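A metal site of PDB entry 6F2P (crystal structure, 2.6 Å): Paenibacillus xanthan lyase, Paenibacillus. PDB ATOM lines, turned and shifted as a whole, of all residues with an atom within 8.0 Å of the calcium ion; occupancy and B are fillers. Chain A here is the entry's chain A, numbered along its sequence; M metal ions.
The side-chain carboxylate (OD1) of Asp 780 sits close to the side-chain hydroxyl (OG1) of Thr 779 (2.9 Å). The side-chain carboxylate (OD1) of Asp 805 lies within hydrogen-bond range of the side-chain hydroxyl (OG1) of Thr 779. N of Ala 802 lies close to OD2 of Asp 805 (3.0 Å). O of Asp 805 sits at hydrogen-bond distance from ND2 of Asn 800 (3.5 Å).
The calcium ion is bound by the side-chain carboxylate of Asp 780, the side-chain amide oxygen of Asn 801 and the side-chain carboxylate of Asp 805. Slightly farther from the calcium ion lies the side-chain carboxylate (OD1) of Asp 805 (2.9 Å).
Within 4 Å of the calcium ion: Asp 780, Asn 801 and Asp 805.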
ATOM      1  N   THR A 779     -25.664  -5.175  28.340  1.00  0.00           N
ATOM      2  CA  THR A 779     -24.677  -4.409  29.106  1.00  0.00           C
ATOM      3  C   THR A 779     -24.384  -3.100  28.409  1.00  0.00           C
ATOM      4  O   THR A 779     -23.987  -2.112  29.024  1.00  0.00           O
ATOM      5  CB  THR A 779     -23.344  -5.154  29.210  1.00  0.00           C
ATOM      6  OG1 THR A 779     -22.762  -5.264  27.907  1.00  0.00           O
ATOM      7  CG2 THR A 779     -23.553  -6.522  29.788  1.00  0.00           C
ATOM      8  N   ASP A 780     -24.564  -3.118  27.088  1.00  0.00           N
ATOM      9  CA  ASP A 780     -24.308  -1.976  26.235  1.00  0.00           C
ATOM     10  C   ASP A 780     -25.460  -1.770  25.269  1.00  0.00           C
ATOM     11  O   ASP A 780     -25.965  -2.740  24.693  1.00  0.00           O
ATOM     12  CB  ASP A 780     -22.998  -2.186  25.468  1.00  0.00           C
ATOM     13  CG  ASP A 780     -21.773  -1.967  26.340  1.00  0.00           C
ATOM     14  OD1 ASP A 780     -21.394  -2.908  27.068  1.00  0.00           O
ATOM     15  OD2 ASP A 780     -21.204  -0.846  26.278  1.00  0.00           O
ATOM     16  N   THR A 781     -25.877  -0.531  25.090  1.00  0.00           N
ATOM     17  CA  THR A 781     -26.983  -0.238  24.184  1.00  0.00           C
ATOM     18  C   THR A 781     -26.572  -0.304  22.711  1.00  0.00           C
ATOM     19  O   THR A 781     -25.660   0.389  22.285  1.00  0.00           O
ATOM     20  CB  THR A 781     -27.597   1.132  24.470  1.00  0.00           C
ATOM     21  OG1 THR A 781     -28.107   1.157  25.801  1.00  0.00           O
ATOM     22  CG2 THR A 781     -28.736   1.429  23.502  1.00  0.00           C
ATOM     23  N   ASN A 799     -22.490  -1.970  20.642  1.00  0.00           N
ATOM     24  CA  ASN A 799     -21.529  -0.972  21.102  1.00  0.00           C
ATOM     25  C   ASN A 799     -20.669  -1.497  22.221  1.00  0.00           C
ATOM     26  O   ASN A 799     -20.074  -0.727  22.976  1.00  0.00           O
ATOM     27  CB  ASN A 799     -22.254   0.302  21.541  1.00  0.00           C
ATOM     28  CG  ASN A 799     -22.748   1.103  20.356  1.00  0.00           C
ATOM     29  OD1 ASN A 799     -21.972   1.450  19.469  1.00  0.00           O
ATOM     30  ND2 ASN A 799     -24.049   1.391  20.334  1.00  0.00           N
ATOM     31  N   ASN A 800     -20.597  -2.820  22.320  1.00  0.00           N
ATOM     32  CA  ASN A 800     -19.876  -3.519  23.370  1.00  0.00           C
ATOM     33  C   ASN A 800     -18.444  -3.030  23.572  1.00  0.00           C
ATOM     34  O   ASN A 800     -17.670  -2.964  22.606  1.00  0.00           O
ATOM     35  CB  ASN A 800     -19.903  -5.019  23.108  1.00  0.00           C
ATOM     36  CG  ASN A 800     -21.323  -5.560  23.017  1.00  0.00           C
ATOM     37  OD1 ASN A 800     -22.230  -4.870  22.552  1.00  0.00           O
ATOM     38  ND2 ASN A 800     -21.525  -6.799  23.468  1.00  0.00           N
ATOM     39  N   ASN A 801     -18.115  -2.696  24.820  1.00  0.00           N
ATOM     40  CA  ASN A 801     -16.851  -2.087  25.231  1.00  0.00           C
ATOM     41  C   ASN A 801     -15.752  -3.087  25.497  1.00  0.00           C
ATOM     42  O   ASN A 801     -14.591  -2.822  25.219  1.00  0.00           O
ATOM     43  CB  ASN A 801     -17.001  -1.328  26.556  1.00  0.00           C
ATOM     44  CG  ASN A 801     -17.989  -0.204  26.477  1.00  0.00           C
ATOM     45  OD1 ASN A 801     -18.893  -0.108  27.306  1.00  0.00           O
ATOM     46  ND2 ASN A 801     -17.803   0.684  25.499  1.00  0.00           N
ATOM     47  N   ALA A 802     -16.126  -4.210  26.093  1.00  0.00           N
ATOM     48  CA  ALA A 802     -15.146  -5.086  26.716  1.00  0.00           C
ATOM     49  C   ALA A 802     -15.622  -6.530  26.766  1.00  0.00           C
ATOM     50  O   ALA A 802     -16.754  -6.833  26.432  1.00  0.00           O
ATOM     51  CB  ALA A 802     -14.832  -4.588  28.122  1.00  0.00           C
ATOM     52  N   VAL A 803     -14.724  -7.413  27.185  1.00  0.00           N
ATOM     53  CA  VAL A 803     -15.036  -8.830  27.318  1.00  0.00           C
ATOM     54  C   VAL A 803     -16.181  -9.022  28.300  1.00  0.00           C
ATOM     55  O   VAL A 803     -16.332  -8.253  29.251  1.00  0.00           O
ATOM     56  CB  VAL A 803     -13.763  -9.618  27.733  1.00  0.00           C
ATOM     57  CG1 VAL A 803     -14.089 -11.049  28.098  1.00  0.00           C
ATOM     58  CG2 VAL A 803     -12.742  -9.570  26.611  1.00  0.00           C
ATOM     59  N   ASP A 804     -17.032 -10.019  28.015  1.00  0.00           N
ATOM     60  CA  ASP A 804     -18.201 -10.358  28.820  1.00  0.00           C
ATOM     61  C   ASP A 804     -19.418  -9.426  28.631  1.00  0.00           C
ATOM     62  O   ASP A 804     -20.478  -9.666  29.212  1.00  0.00           O
ATOM     63  CB  ASP A 804     -17.841 -10.546  30.289  1.00  0.00           C
ATOM     64  CG  ASP A 804     -17.069 -11.819  30.528  1.00  0.00           C
ATOM     65  OD1 ASP A 804     -17.239 -12.777  29.732  1.00  0.00           O
ATOM     66  OD2 ASP A 804     -16.293 -11.879  31.504  1.00  0.00           O
ATOM     67  N   ASP A 805     -19.248  -8.382  27.831  1.00  0.00           N
ATOM     68  CA  ASP A 805     -20.384  -7.583  27.385  1.00  0.00           C
ATOM     69  C   ASP A 805     -21.278  -8.456  26.527  1.00  0.00           C
ATOM     70  O   ASP A 805     -20.796  -9.288  25.748  1.00  0.00           O
ATOM     71  CB  ASP A 805     -19.918  -6.385  26.550  1.00  0.00           C
ATOM     72  CG  ASP A 805     -19.570  -5.176  27.405  1.00  0.00           C
ATOM     73  OD1 ASP A 805     -19.882  -5.167  28.618  1.00  0.00           O
ATOM     74  OD2 ASP A 805     -19.010  -4.219  26.825  1.00  0.00           O
ATOM     75  N   TYR A 806     -22.593  -8.289  26.668  1.00  0.00           N
ATOM     76  CA  TYR A 806     -23.517  -9.092  25.892  1.00  0.00           C
ATOM     77  C   TYR A 806     -24.776  -8.338  25.517  1.00  0.00           C
ATOM     78  O   TYR A 806     -25.051  -7.263  26.055  1.00  0.00           O
ATOM     79  CB  TYR A 806     -23.882 -10.371  26.663  1.00  0.00           C
ATOM     80  CG  TYR A 806     -24.646 -10.117  27.928  1.00  0.00           C
ATOM     81  CD1 TYR A 806     -26.035 -10.056  27.925  1.00  0.00           C
ATOM     82  CD2 TYR A 806     -23.987  -9.939  29.146  1.00  0.00           C
ATOM     83  CE1 TYR A 806     -26.742  -9.806  29.082  1.00  0.00           C
ATOM     84  CE2 TYR A 806     -24.687  -9.705  30.303  1.00  0.00           C
ATOM     85  CZ  TYR A 806     -26.063  -9.631  30.271  1.00  0.00           C
ATOM     86  OH  TYR A 806     -26.776  -9.400  31.420  1.00  0.00           O
HETATM   87 CA    CA M   1     -19.513  -2.263  28.534  1.00  0.00          CA
